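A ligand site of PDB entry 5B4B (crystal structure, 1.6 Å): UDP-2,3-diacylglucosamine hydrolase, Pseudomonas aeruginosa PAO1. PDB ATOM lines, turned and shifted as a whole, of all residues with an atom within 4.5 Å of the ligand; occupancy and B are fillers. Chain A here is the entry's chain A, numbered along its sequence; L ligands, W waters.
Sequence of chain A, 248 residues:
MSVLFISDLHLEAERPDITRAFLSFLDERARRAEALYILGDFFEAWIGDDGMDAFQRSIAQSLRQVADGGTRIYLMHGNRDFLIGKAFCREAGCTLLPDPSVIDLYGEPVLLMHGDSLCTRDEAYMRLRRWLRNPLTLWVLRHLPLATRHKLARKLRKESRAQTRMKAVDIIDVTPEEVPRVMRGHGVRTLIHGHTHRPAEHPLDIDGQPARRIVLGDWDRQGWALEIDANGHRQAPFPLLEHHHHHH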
ATOM      1  N   GLU A  44      -2.690  15.673  30.683  1.00  0.00           N
ATOM      2  CA  GLU A  44      -3.089  17.058  30.422  1.00  0.00           C
ATOM      3  C   GLU A  44      -1.882  17.966  30.277  1.00  0.00           C
ATOM      4  O   GLU A  44      -1.903  18.945  29.522  1.00  0.00           O
ATOM      5  CB  GLU A  44      -4.014  17.542  31.527  1.00  0.00           C
ATOM      6  CG  GLU A  44      -4.587  18.908  31.312  1.00  0.00           C
ATOM      7  CD  GLU A  44      -3.687  20.042  31.752  1.00  0.00           C
ATOM      8  OE1 GLU A  44      -2.823  19.870  32.642  1.00  0.00           O
ATOM      9  OE2 GLU A  44      -3.874  21.142  31.204  1.00  0.00           O
ATOM     10  N   ALA A  45      -0.820  17.679  31.023  1.00  0.00           N
ATOM     11  CA  ALA A  45       0.418  18.432  30.948  1.00  0.00           C
ATOM     12  C   ALA A  45       1.511  17.578  31.570  1.00  0.00           C
ATOM     13  O   ALA A  45       1.226  16.654  32.353  1.00  0.00           O
ATOM     14  CB  ALA A  45       0.311  19.767  31.680  1.00  0.00           C
ATOM     15  N   TRP A  46       2.768  17.850  31.188  1.00  0.00           N
ATOM     16  CA  TRP A  46       3.944  17.235  31.808  1.00  0.00           C
ATOM     17  C   TRP A  46       5.014  18.303  31.985  1.00  0.00           C
ATOM     18  O   TRP A  46       5.377  18.933  30.996  1.00  0.00           O
ATOM     19  CB  TRP A  46       4.544  16.115  30.963  1.00  0.00           C
ATOM     20  CG  TRP A  46       5.427  15.164  31.738  1.00  0.00           C
ATOM     21  CD1 TRP A  46       6.801  15.055  31.692  1.00  0.00           C
ATOM     22  CD2 TRP A  46       4.983  14.135  32.618  1.00  0.00           C
ATOM     23  NE1 TRP A  46       7.223  14.042  32.528  1.00  0.00           N
ATOM     24  CE2 TRP A  46       6.118  13.462  33.104  1.00  0.00           C
ATOM     25  CE3 TRP A  46       3.714  13.722  33.052  1.00  0.00           C
ATOM     26  CZ2 TRP A  46       6.021  12.410  33.994  1.00  0.00           C
ATOM     27  CZ3 TRP A  46       3.645  12.658  33.935  1.00  0.00           C
ATOM     28  CH2 TRP A  46       4.778  12.034  34.380  1.00  0.00           C
ATOM     29  N   ILE A  47       5.496  18.494  33.216  1.00  0.00           N
ATOM     30  CA  ILE A  47       6.513  19.505  33.454  1.00  0.00           C
ATOM     31  C   ILE A  47       7.909  18.901  33.590  1.00  0.00           C
ATOM     32  O   ILE A  47       8.867  19.611  33.915  1.00  0.00           O
ATOM     33  CB  ILE A  47       6.164  20.380  34.673  1.00  0.00           C
ATOM     34  CG1 ILE A  47       6.096  19.551  35.967  1.00  0.00           C
ATOM     35  CG2 ILE A  47       4.865  21.177  34.416  1.00  0.00           C
ATOM     36  CD1 ILE A  47       6.323  20.387  37.220  1.00  0.00           C
ATOM     37  N   ASN A  79       1.925  17.496  22.209  1.00  0.00           N
ATOM     38  CA  ASN A  79       2.208  18.882  22.544  1.00  0.00           C
ATOM     39  C   ASN A  79       2.027  19.189  24.025  1.00  0.00           C
ATOM     40  O   ASN A  79       2.555  20.188  24.501  1.00  0.00           O
ATOM     41  CB  ASN A  79       1.333  19.797  21.691  1.00  0.00           C
ATOM     42  CG  ASN A  79      -0.107  19.502  21.853  1.00  0.00           C
ATOM     43  OD1 ASN A  79      -0.553  18.422  21.507  1.00  0.00           O
ATOM     44  ND2 ASN A  79      -0.860  20.440  22.372  1.00  0.00           N
ATOM     45  N   ARG A  80       1.272  18.358  24.773  1.00  0.00           N
ATOM     46  CA  ARG A  80       1.087  18.540  26.208  1.00  0.00           C
ATOM     47  C   ARG A  80       2.190  17.905  27.011  1.00  0.00           C
ATOM     48  O   ARG A  80       2.499  18.379  28.117  1.00  0.00           O
ATOM     49  CB  ARG A  80      -0.225  17.886  26.667  1.00  0.00           C
ATOM     50  CG  ARG A  80      -1.468  18.455  26.059  1.00  0.00           C
ATOM     51  CD  ARG A  80      -1.593  19.892  26.331  1.00  0.00           C
ATOM     52  NE  ARG A  80      -2.876  20.338  25.817  1.00  0.00           N
ATOM     53  CZ  ARG A  80      -4.015  20.155  26.467  1.00  0.00           C
ATOM     54  NH1 ARG A  80      -4.034  19.563  27.650  1.00  0.00           N
ATOM     55  NH2 ARG A  80      -5.151  20.566  25.907  1.00  0.00           N
ATOM     56  N   PHE A  82       5.439  16.451  25.816  1.00  0.00           N
ATOM     57  CA  PHE A  82       6.713  16.224  25.137  1.00  0.00           C
ATOM     58  C   PHE A  82       7.905  16.166  26.098  1.00  0.00           C
ATOM     59  O   PHE A  82       8.978  15.733  25.671  1.00  0.00           O
ATOM     60  CB  PHE A  82       6.948  17.312  24.073  1.00  0.00           C
ATOM     61  CG  PHE A  82       6.982  18.680  24.617  1.00  0.00           C
ATOM     62  CD1 PHE A  82       5.815  19.410  24.790  1.00  0.00           C
ATOM     63  CD2 PHE A  82       8.183  19.247  25.026  1.00  0.00           C
ATOM     64  CE1 PHE A  82       5.847  20.654  25.369  1.00  0.00           C
ATOM     65  CE2 PHE A  82       8.231  20.512  25.574  1.00  0.00           C
ATOM     66  CZ  PHE A  82       7.067  21.222  25.767  1.00  0.00           C
ATOM     67  N   LEU A  83       7.731  16.601  27.352  1.00  0.00           N
ATOM     68  CA  LEU A  83       8.821  16.476  28.310  1.00  0.00           C
ATOM     69  C   LEU A  83       8.919  15.097  28.942  1.00  0.00           C
ATOM     70  O   LEU A  83       9.852  14.879  29.715  1.00  0.00           O
ATOM     71  CB  LEU A  83       8.690  17.545  29.393  1.00  0.00           C
ATOM     72  CG  LEU A  83       8.977  18.979  28.886  1.00  0.00           C
ATOM     73  CD1 LEU A  83       8.694  19.990  29.961  1.00  0.00           C
ATOM     74  CD2 LEU A  83      10.407  19.186  28.403  1.00  0.00           C
ATOM     75  N   ASP A 122      -0.785  26.540  10.779  1.00  0.00           N
ATOM     76  CA  ASP A 122      -0.921  27.227  12.072  1.00  0.00           C
ATOM     77  C   ASP A 122       0.446  27.826  12.431  1.00  0.00           C
ATOM     78  O   ASP A 122       1.232  27.253  13.198  1.00  0.00           O
ATOM     79  CB  ASP A 122      -1.403  26.239  13.120  1.00  0.00           C
ATOM     80  CG  ASP A 122      -1.832  26.887  14.434  1.00  0.00           C
ATOM     81  OD1 ASP A 122      -1.549  28.080  14.644  1.00  0.00           O
ATOM     82  OD2 ASP A 122      -2.465  26.142  15.222  1.00  0.00           O
ATOM     83  N   ALA A 124       1.562  30.416  14.136  1.00  0.00           N
ATOM     84  CA  ALA A 124       1.911  30.739  15.519  1.00  0.00           C
ATOM     85  C   ALA A 124       2.248  29.480  16.300  1.00  0.00           C
ATOM     86  O   ALA A 124       3.178  29.465  17.108  1.00  0.00           O
ATOM     87  CB  ALA A 124       0.777  31.497  16.192  1.00  0.00           C
ATOM     88  N   TYR A 125       1.485  28.409  16.077  1.00  0.00           N
ATOM     89  CA  TYR A 125       1.799  27.152  16.743  1.00  0.00           C
ATOM     90  C   TYR A 125       3.128  26.601  16.243  1.00  0.00           C
ATOM     91  O   TYR A 125       3.927  26.067  17.018  1.00  0.00           O
ATOM     92  CB  TYR A 125       0.678  26.116  16.564  1.00  0.00           C
ATOM     93  CG  TYR A 125       1.113  24.827  17.200  1.00  0.00           C
ATOM     94  CD1 TYR A 125       1.363  24.762  18.557  1.00  0.00           C
ATOM     95  CD2 TYR A 125       1.407  23.694  16.435  1.00  0.00           C
ATOM     96  CE1 TYR A 125       1.862  23.646  19.137  1.00  0.00           C
ATOM     97  CE2 TYR A 125       1.913  22.545  17.031  1.00  0.00           C
ATOM     98  CZ  TYR A 125       2.125  22.528  18.392  1.00  0.00           C
ATOM     99  OH  TYR A 125       2.627  21.419  19.029  1.00  0.00           O
ATOM    100  N   LEU A 128       5.851  28.282  18.028  1.00  0.00           N
ATOM    101  CA  LEU A 128       5.924  27.800  19.402  1.00  0.00           C
ATOM    102  C   LEU A 128       6.568  26.418  19.479  1.00  0.00           C
ATOM    103  O   LEU A 128       7.407  26.144  20.351  1.00  0.00           O
ATOM    104  CB  LEU A 128       4.511  27.781  20.023  1.00  0.00           C
ATOM    105  CG  LEU A 128       4.417  27.166  21.426  1.00  0.00           C
ATOM    106  CD1 LEU A 128       5.071  28.039  22.506  1.00  0.00           C
ATOM    107  CD2 LEU A 128       2.964  26.918  21.790  1.00  0.00           C
ATOM    108  N   TRP A 131      10.300  26.353  18.980  1.00  0.00           N
ATOM    109  CA  TRP A 131      10.982  26.850  20.179  1.00  0.00           C
ATOM    110  C   TRP A 131      10.946  25.819  21.304  1.00  0.00           C
ATOM    111  O   TRP A 131      11.957  25.540  21.965  1.00  0.00           O
ATOM    112  CB  TRP A 131      10.324  28.161  20.609  1.00  0.00           C
ATOM    113  CG  TRP A 131      10.906  28.726  21.841  1.00  0.00           C
ATOM    114  CD1 TRP A 131      12.092  29.377  21.963  1.00  0.00           C
ATOM    115  CD2 TRP A 131      10.347  28.650  23.147  1.00  0.00           C
ATOM    116  NE1 TRP A 131      12.301  29.738  23.283  1.00  0.00           N
ATOM    117  CE2 TRP A 131      11.239  29.307  24.024  1.00  0.00           C
ATOM    118  CE3 TRP A 131       9.160  28.117  23.660  1.00  0.00           C
ATOM    119  CZ2 TRP A 131      10.988  29.428  25.387  1.00  0.00           C
ATOM    120  CZ3 TRP A 131       8.900  28.252  25.018  1.00  0.00           C
ATOM    121  CH2 TRP A 131       9.804  28.899  25.863  1.00  0.00           C
ATOM    122  N   LEU A 132       9.778  25.240  21.566  1.00  0.00           N
ATOM    123  CA  LEU A 132       9.687  24.308  22.687  1.00  0.00           C
ATOM    124  C   LEU A 132      10.613  23.119  22.507  1.00  0.00           C
ATOM    125  O   LEU A 132      11.122  22.575  23.504  1.00  0.00           O
ATOM    126  CB  LEU A 132       8.253  23.812  22.838  1.00  0.00           C
ATOM    127  CG  LEU A 132       7.242  24.747  23.501  1.00  0.00           C
ATOM    128  CD1 LEU A 132       5.811  24.159  23.334  1.00  0.00           C
ATOM    129  CD2 LEU A 132       7.623  24.982  24.962  1.00  0.00           C
ATOM    130  N   LEU A 141      13.893  24.386  30.477  1.00  0.00           N
ATOM    131  CA  LEU A 141      12.611  24.087  31.119  1.00  0.00           C
ATOM    132  C   LEU A 141      12.780  23.002  32.161  1.00  0.00           C
ATOM    133  O   LEU A 141      12.144  23.042  33.220  1.00  0.00           O
ATOM    134  CB  LEU A 141      11.573  23.653  30.083  1.00  0.00           C
ATOM    135  CG  LEU A 141      11.104  24.708  29.103  1.00  0.00           C
ATOM    136  CD1 LEU A 141      10.126  24.034  28.088  1.00  0.00           C
ATOM    137  CD2 LEU A 141      10.443  25.868  29.824  1.00  0.00           C
ATOM    138  N   ARG A 149       7.825  26.061  36.789  1.00  0.00           N
ATOM    139  CA  ARG A 149       7.339  25.255  35.674  1.00  0.00           C
ATOM    140  C   ARG A 149       5.825  25.224  35.638  1.00  0.00           C
ATOM    141  O   ARG A 149       5.209  25.333  34.580  1.00  0.00           O
ATOM    142  CB  ARG A 149       7.885  23.827  35.758  1.00  0.00           C
ATOM    143  CG  ARG A 149       9.372  23.742  35.528  1.00  0.00           C
ATOM    144  CD  ARG A 149       9.856  22.314  35.438  1.00  0.00           C
ATOM    145  NE  ARG A 149      10.931  22.041  36.390  1.00  0.00           N
ATOM    146  CZ  ARG A 149      11.455  20.842  36.558  1.00  0.00           C
ATOM    147  NH1 ARG A 149      10.991  19.816  35.865  1.00  0.00           N
ATOM    148  NH2 ARG A 149      12.442  20.661  37.443  1.00  0.00           N
ATOM    149  N   LEU A 152       4.605  28.547  34.281  1.00  0.00           N
ATOM    150  CA  LEU A 152       4.780  28.641  32.833  1.00  0.00           C
ATOM    151  C   LEU A 152       3.758  27.766  32.106  1.00  0.00           C
ATOM    152  O   LEU A 152       3.225  28.149  31.060  1.00  0.00           O
ATOM    153  CB  LEU A 152       6.206  28.262  32.445  1.00  0.00           C
ATOM    154  CG  LEU A 152       7.324  29.196  32.955  1.00  0.00           C
ATOM    155  CD1 LEU A 152       8.674  28.703  32.460  1.00  0.00           C
ATOM    156  CD2 LEU A 152       7.090  30.608  32.527  1.00  0.00           C
ATOM    157  N   ALA A 153       3.507  26.559  32.627  1.00  0.00           N
ATOM    158  CA  ALA A 153       2.546  25.662  31.990  1.00  0.00           C
ATOM    159  C   ALA A 153       1.150  26.275  31.985  1.00  0.00           C
ATOM    160  O   ALA A 153       0.449  26.228  30.961  1.00  0.00           O
ATOM    161  CB  ALA A 153       2.533  24.312  32.727  1.00  0.00           C
ATOM    162  N   LYS A 155       0.408  29.461  32.072  1.00  0.00           N
ATOM    163  CA  LYS A 155       0.440  30.564  31.122  1.00  0.00           C
ATOM    164  C   LYS A 155       0.273  30.060  29.703  1.00  0.00           C
ATOM    165  O   LYS A 155      -0.483  30.628  28.905  1.00  0.00           O
ATOM    166  CB  LYS A 155       1.766  31.312  31.263  1.00  0.00           C
ATOM    167  CG  LYS A 155       2.072  32.310  30.159  1.00  0.00           C
ATOM    168  CD  LYS A 155       1.105  33.473  30.197  1.00  0.00           C
ATOM    169  CE  LYS A 155       1.415  34.458  29.089  1.00  0.00           C
ATOM    170  NZ  LYS A 155       0.442  35.577  29.114  1.00  0.00           N
ATOM    171  N   LEU A 156       1.012  29.024  29.358  1.00  0.00           N
ATOM    172  CA  LEU A 156       0.931  28.453  28.022  1.00  0.00           C
ATOM    173  C   LEU A 156      -0.472  27.925  27.750  1.00  0.00           C
ATOM    174  O   LEU A 156      -1.024  28.146  26.663  1.00  0.00           O
ATOM    175  CB  LEU A 156       2.004  27.373  27.881  1.00  0.00           C
ATOM    176  CG  LEU A 156       2.141  26.710  26.531  1.00  0.00           C
ATOM    177  CD1 LEU A 156       2.222  27.733  25.402  1.00  0.00           C
ATOM    178  CD2 LEU A 156       3.398  25.862  26.549  1.00  0.00           C
ATOM    179  N   ARG A 157      -1.074  27.228  28.725  1.00  0.00           N
ATOM    180  CA  ARG A 157      -2.432  26.724  28.522  1.00  0.00           C
ATOM    181  C   ARG A 157      -3.405  27.863  28.315  1.00  0.00           C
ATOM    182  O   ARG A 157      -4.288  27.795  27.446  1.00  0.00           O
ATOM    183  CB  ARG A 157      -2.909  25.934  29.740  1.00  0.00           C
ATOM    184  CG  ARG A 157      -2.285  24.614  30.035  1.00  0.00           C
ATOM    185  CD  ARG A 157      -3.150  23.960  31.150  1.00  0.00           C
ATOM    186  NE  ARG A 157      -2.495  22.958  31.976  1.00  0.00           N
ATOM    187  CZ  ARG A 157      -1.824  23.171  33.082  1.00  0.00           C
ATOM    188  NH1 ARG A 157      -1.739  24.399  33.557  1.00  0.00           N
ATOM    189  NH2 ARG A 157      -1.223  22.187  33.731  1.00  0.00           N
ATOM    190  N   GLU A 159      -2.897  31.001  27.309  1.00  0.00           N
ATOM    191  CA  GLU A 159      -2.745  31.685  26.019  1.00  0.00           C
ATOM    192  C   GLU A 159      -3.164  30.780  24.865  1.00  0.00           C
ATOM    193  O   GLU A 159      -3.710  31.262  23.860  1.00  0.00           O
ATOM    194  CB  GLU A 159      -1.314  32.144  25.832  1.00  0.00           C
ATOM    195  CG  GLU A 159      -0.882  33.186  26.840  1.00  0.00           C
ATOM    196  CD  GLU A 159      -1.825  34.372  26.878  1.00  0.00           C
ATOM    197  OE1 GLU A 159      -2.331  34.747  25.780  1.00  0.00           O
ATOM    198  OE2 GLU A 159      -2.071  34.902  27.987  1.00  0.00           O
ATOM    199  N   SER A 160      -2.885  29.488  24.972  1.00  0.00           N
ATOM    200  CA  SER A 160      -3.277  28.574  23.906  1.00  0.00           C
ATOM    201  C   SER A 160      -4.798  28.530  23.769  1.00  0.00           C
ATOM    202  O   SER A 160      -5.326  28.663  22.670  1.00  0.00           O
ATOM    203  CB  SER A 160      -2.731  27.181  24.159  1.00  0.00           C
ATOM    204  OG  SER A 160      -3.370  26.229  23.321  1.00  0.00           O
ATOM    205  N   GLN A 163      -5.959  31.775  22.049  1.00  0.00           N
ATOM    206  CA  GLN A 163      -5.633  31.853  20.626  1.00  0.00           C
ATOM    207  C   GLN A 163      -6.395  30.803  19.817  1.00  0.00           C
ATOM    208  O   GLN A 163      -6.898  31.113  18.734  1.00  0.00           O
ATOM    209  CB  GLN A 163      -4.133  31.702  20.428  1.00  0.00           C
ATOM    210  CG  GLN A 163      -3.332  32.929  20.843  1.00  0.00           C
ATOM    211  CD  GLN A 163      -2.003  33.061  20.086  1.00  0.00           C
ATOM    212  OE1 GLN A 163      -1.896  32.686  18.901  1.00  0.00           O
ATOM    213  NE2 GLN A 163      -0.987  33.591  20.757  1.00  0.00           N
ATOM    214  N   THR A 164      -6.527  29.579  20.334  1.00  0.00           N
ATOM    215  CA  THR A 164      -7.185  28.525  19.568  1.00  0.00           C
ATOM    216  C   THR A 164      -8.649  28.855  19.305  1.00  0.00           C
ATOM    217  O   THR A 164      -9.164  28.580  18.226  1.00  0.00           O
ATOM    218  CB  THR A 164      -7.031  27.168  20.285  1.00  0.00           C
ATOM    219  OG1 THR A 164      -5.632  26.835  20.412  1.00  0.00           O
ATOM    220  CG2 THR A 164      -7.704  26.055  19.522  1.00  0.00           C
ATOM    221  N   LYS A 167      -9.028  30.541  15.916  1.00  0.00           N
ATOM    222  CA  LYS A 167      -8.457  29.929  14.730  1.00  0.00           C
ATOM    223  C   LYS A 167      -9.510  29.063  14.047  1.00  0.00           C
ATOM    224  O   LYS A 167     -10.107  28.191  14.672  1.00  0.00           O
ATOM    225  CB  LYS A 167      -7.251  29.066  15.095  1.00  0.00           C
ATOM    226  CG  LYS A 167      -6.100  29.817  15.719  1.00  0.00           C
ATOM    227  CD  LYS A 167      -4.971  28.833  16.083  1.00  0.00           C
ATOM    228  CE  LYS A 167      -3.903  29.521  16.927  1.00  0.00           C
ATOM    229  NZ  LYS A 167      -2.731  28.608  17.083  1.00  0.00           N
ATOM    230  N   ILE A 172      -6.035  24.956  12.123  1.00  0.00           N
ATOM    231  CA  ILE A 172      -5.499  24.052  13.125  1.00  0.00           C
ATOM    232  C   ILE A 172      -5.427  22.591  12.695  1.00  0.00           C
ATOM    233  O   ILE A 172      -4.639  21.860  13.292  1.00  0.00           O
ATOM    234  CB  ILE A 172      -6.263  24.153  14.457  1.00  0.00           C
ATOM    235  CG1 ILE A 172      -7.736  23.815  14.306  1.00  0.00           C
ATOM    236  CG2 ILE A 172      -6.084  25.574  15.023  1.00  0.00           C
ATOM    237  CD1 ILE A 172      -8.429  23.747  15.660  1.00  0.00           C
ATOM    238  N   HIS A 195      -4.004  14.363  17.944  1.00  0.00           N
ATOM    239  CA  HIS A 195      -3.886  15.805  18.045  1.00  0.00           C
ATOM    240  C   HIS A 195      -5.140  16.595  17.644  1.00  0.00           C
ATOM    241  O   HIS A 195      -5.506  17.551  18.340  1.00  0.00           O
ATOM    242  CB  HIS A 195      -2.699  16.353  17.264  1.00  0.00           C
ATOM    243  CG  HIS A 195      -2.504  17.780  17.552  1.00  0.00           C
ATOM    244  ND1 HIS A 195      -2.097  18.232  18.784  1.00  0.00           N
ATOM    245  CD2 HIS A 195      -2.747  18.887  16.815  1.00  0.00           C
ATOM    246  CE1 HIS A 195      -2.074  19.548  18.801  1.00  0.00           C
ATOM    247  NE2 HIS A 195      -2.468  19.973  17.616  1.00  0.00           N
HETATM  248  O1  LIG L   1      -5.192  21.718  23.032  1.00  0.00           O
HETATM  249  P1  LIG L   1      -4.122  22.734  23.228  1.00  0.00           P
HETATM  250  O2  LIG L   1      -4.576  23.913  24.072  1.00  0.00           O
HETATM  251  O3  LIG L   1      -2.773  22.133  23.627  1.00  0.00           O
HETATM  252  O4  LIG L   1      -3.899  23.381  21.738  1.00  0.00           O
HETATM  253  C1  LIG L   1      -2.827  22.986  20.905  1.00  0.00           C
HETATM  254  C2  LIG L   1      -1.816  24.106  20.831  1.00  0.00           C
HETATM  255  N1  LIG L   1      -1.322  24.488  22.132  1.00  0.00           N
HETATM  256  C3  LIG L   1      -0.231  23.962  22.672  1.00  0.00           C
HETATM  257  C4  LIG L   1       0.124  24.486  24.026  1.00  0.00           C
HETATM  258  C5  LIG L   1       0.063  23.268  24.923  1.00  0.00           C
HETATM  259  O5  LIG L   1      -1.282  23.185  25.379  1.00  0.00           O
HETATM  260  C6  LIG L   1       1.065  23.388  26.030  1.00  0.00           C
HETATM  261  C7  LIG L   1       0.405  23.876  27.316  1.00  0.00           C
HETATM  262  C8  LIG L   1      -0.060  22.673  28.143  1.00  0.00           C
HETATM  263  C9  LIG L   1       0.951  22.350  29.234  1.00  0.00           C
HETATM  264  C10 LIG L   1       2.239  22.014  28.523  1.00  0.00           C
HETATM  265  C11 LIG L   1       3.380  21.404  29.305  1.00  0.00           C
HETATM  266  C12 LIG L   1       4.696  22.000  28.838  1.00  0.00           C
HETATM  267  C13 LIG L   1       5.302  22.710  30.011  1.00  0.00           C
HETATM  268  C14 LIG L   1       6.369  23.682  29.605  1.00  0.00           C
HETATM  269  C15 LIG L   1       6.768  24.534  30.790  1.00  0.00           C
HETATM  270  C16 LIG L   1       7.474  23.710  31.850  1.00  0.00           C
HETATM  271  O6  LIG L   1       0.453  23.128  22.147  1.00  0.00           O
HETATM  272  C17 LIG L   1      -2.405  25.298  20.137  1.00  0.00           C
HETATM  273  C18 LIG L   1      -2.801  24.881  18.737  1.00  0.00           C
HETATM  274  C19 LIG L   1      -3.825  23.764  18.867  1.00  0.00           C
HETATM  275  O7  LIG L   1      -3.245  22.675  19.565  1.00  0.00           O
HETATM  276  C20 LIG L   1      -4.282  23.239  17.517  1.00  0.00           C
HETATM  277  O8  LIG L   1      -3.146  22.570  16.934  1.00  0.00           O
HETATM  278  O9  LIG L   1      -3.384  25.983  18.042  1.00  0.00           O
HETATM  279  O10 LIG L   1      -1.344  26.226  20.012  1.00  0.00           O
HETATM  280  C21 LIG L   1      -1.592  27.605  20.281  1.00  0.00           C
HETATM  281  O11 LIG L   1      -2.717  28.021  20.444  1.00  0.00           O
HETATM  282  C22 LIG L   1      -0.303  28.408  20.322  1.00  0.00           C
HETATM  283  C23 LIG L   1      -0.577  29.896  20.149  1.00  0.00           C
HETATM  284  O12 LIG L   1      -0.981  30.114  18.796  1.00  0.00           O
HETATM  285  C24 LIG L   1       0.695  30.686  20.492  1.00  0.00           C
HETATM  286  C25 LIG L   1       0.937  30.735  22.006  1.00  0.00           C
HETATM  287  C26 LIG L   1       2.180  31.519  22.448  1.00  0.00           C
HETATM  288  C27 LIG L   1       2.348  31.369  23.963  1.00  0.00           C
HETATM  289  C28 LIG L   1       3.401  32.247  24.577  1.00  0.00           C
HETATM  290  C29 LIG L   1       3.637  32.062  26.047  1.00  0.00           C
HETATM  291  C30 LIG L   1       4.610  30.916  26.360  1.00  0.00           C
HETATM  292  C31 LIG L   1       5.247  31.011  27.744  1.00  0.00           C
HETATM  293  C32 LIG L   1       6.407  30.036  27.891  1.00  0.00           C
HETATM  294  C33 LIG L   1       5.956  28.582  28.026  1.00  0.00           C
HETATM  295  C34 LIG L   1       7.131  27.690  28.406  1.00  0.00           C
HETATM  296  O   HOH W   1      -7.365  24.093  23.658  1.00  0.00           O
HETATM  297  O   HOH W   2      -5.380  20.179  19.523  1.00  0.00           O
HETATM  298  O   HOH W   3       2.904  22.618  23.213  1.00  0.00           O
HETATM  299  O   HOH W   4      -2.576  23.416  14.749  1.00  0.00           O
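Water W4 lies within hydrogen-bond range of O8 of the ligand (2.4 Å), OD2 of Asp 122 (2.8 Å) and O of Ile 172 (3.0 Å).
Water W3 lies within hydrogen-bond range of O6 of the ligand and O of Asn 79.
Water W2 lies within hydrogen-bond range of the backbone carbonyl oxygen of His 195 (2.9 Å) and an oxygen (O7) of the ligand (3.3 Å).
The side-chain amino group (NZ) of Lys 167 is in hydrogen-bond range of an oxygen (O9) of the ligand, at 2.9 Å.
OG1 of Thr 164 is in hydrogen-bond range of O11 of the ligand, at 3.1 Å.
The side-chain amide oxygen of Gln 163 lies within hydrogen-bond range of an oxygen (O12) of the ligand.
OD2 of Asp 122 lies within hydrogen-bond range of O9 of the ligand (3.0 Å).
An oxygen (O8) of the ligand lies within hydrogen-bond range of a ring nitrogen (NE2) of His 195, 2.8 Å away.
O3 of the ligand lies within salt-bridge range of NE of Arg 80 (2.8 Å).
ND2 of Asn 79 is in hydrogen-bond range of O3 of the ligand.
OG of Ser 160 sits at hydrogen-bond distance from O2 of the ligand (2.7 Å).
Ala 45 touches the ligand (CB to C9, 3.6 Å).
O of Trp 46 touches C11 of the ligand (3.6 Å).
Phe 82 touches the ligand.
Ala 124 touches the ligand (CB to O12, 3.4 Å).
Tyr 125 touches the ligand (CE1 to O6, 3.4 Å).
Leu 128 touches the ligand (CD2 to C22, 3.9 Å).
CZ3 of Trp 131 touches C34 of the ligand, 3.9 Å away.
Arg 149 touches the ligand (O to C16, 3.9 Å).
Leu 156 touches the ligand.
Arg 157 touches the ligand.
CB of Ile 172 touches C20 of the ligand (3.8 Å).
Hydrophobic or aromatic side chains within 4 Å of the ligand: Ala 45, Phe 82, Ala 124, Tyr 125, Leu 128, Trp 131, Leu 156, Ile 172 and His 195.
Of the 28 residues printed, 19 come within 4 Å of the ligand.
The backbone carbonyl oxygen (O) of Ser 160 is in hydrogen-bond range of the side-chain hydroxyl (OG1) of Thr 164 (2.9 Å).
NH1 of Arg 80 lies within salt-bridge range of OE2 of Glu 44 (3.9 Å).
The guanidinium group (NE) of Arg 157 lies within salt-bridge range of the side-chain carboxylate (OE2) of Glu 44, at 2.4 Å.
The side-chain amino group (NZ) of Lys 167 is in salt-bridge range of the side-chain carboxylate (OD1) of Asp 122, 2.8 Å away.
OD1 of Asp 122 is in hydrogen-bond range of N of Tyr 125.
ND1 of His 195 is in hydrogen-bond range of OD1 of Asn 79, 3.1 Å away.
NH1 of Arg 149 sits at hydrogen-bond distance from O of Ile 47 (2.9 Å).
The backbone carbonyl oxygen of Arg 80 lies within hydrogen-bond range of the backbone NH of Trp 46, 3.1 Å away.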
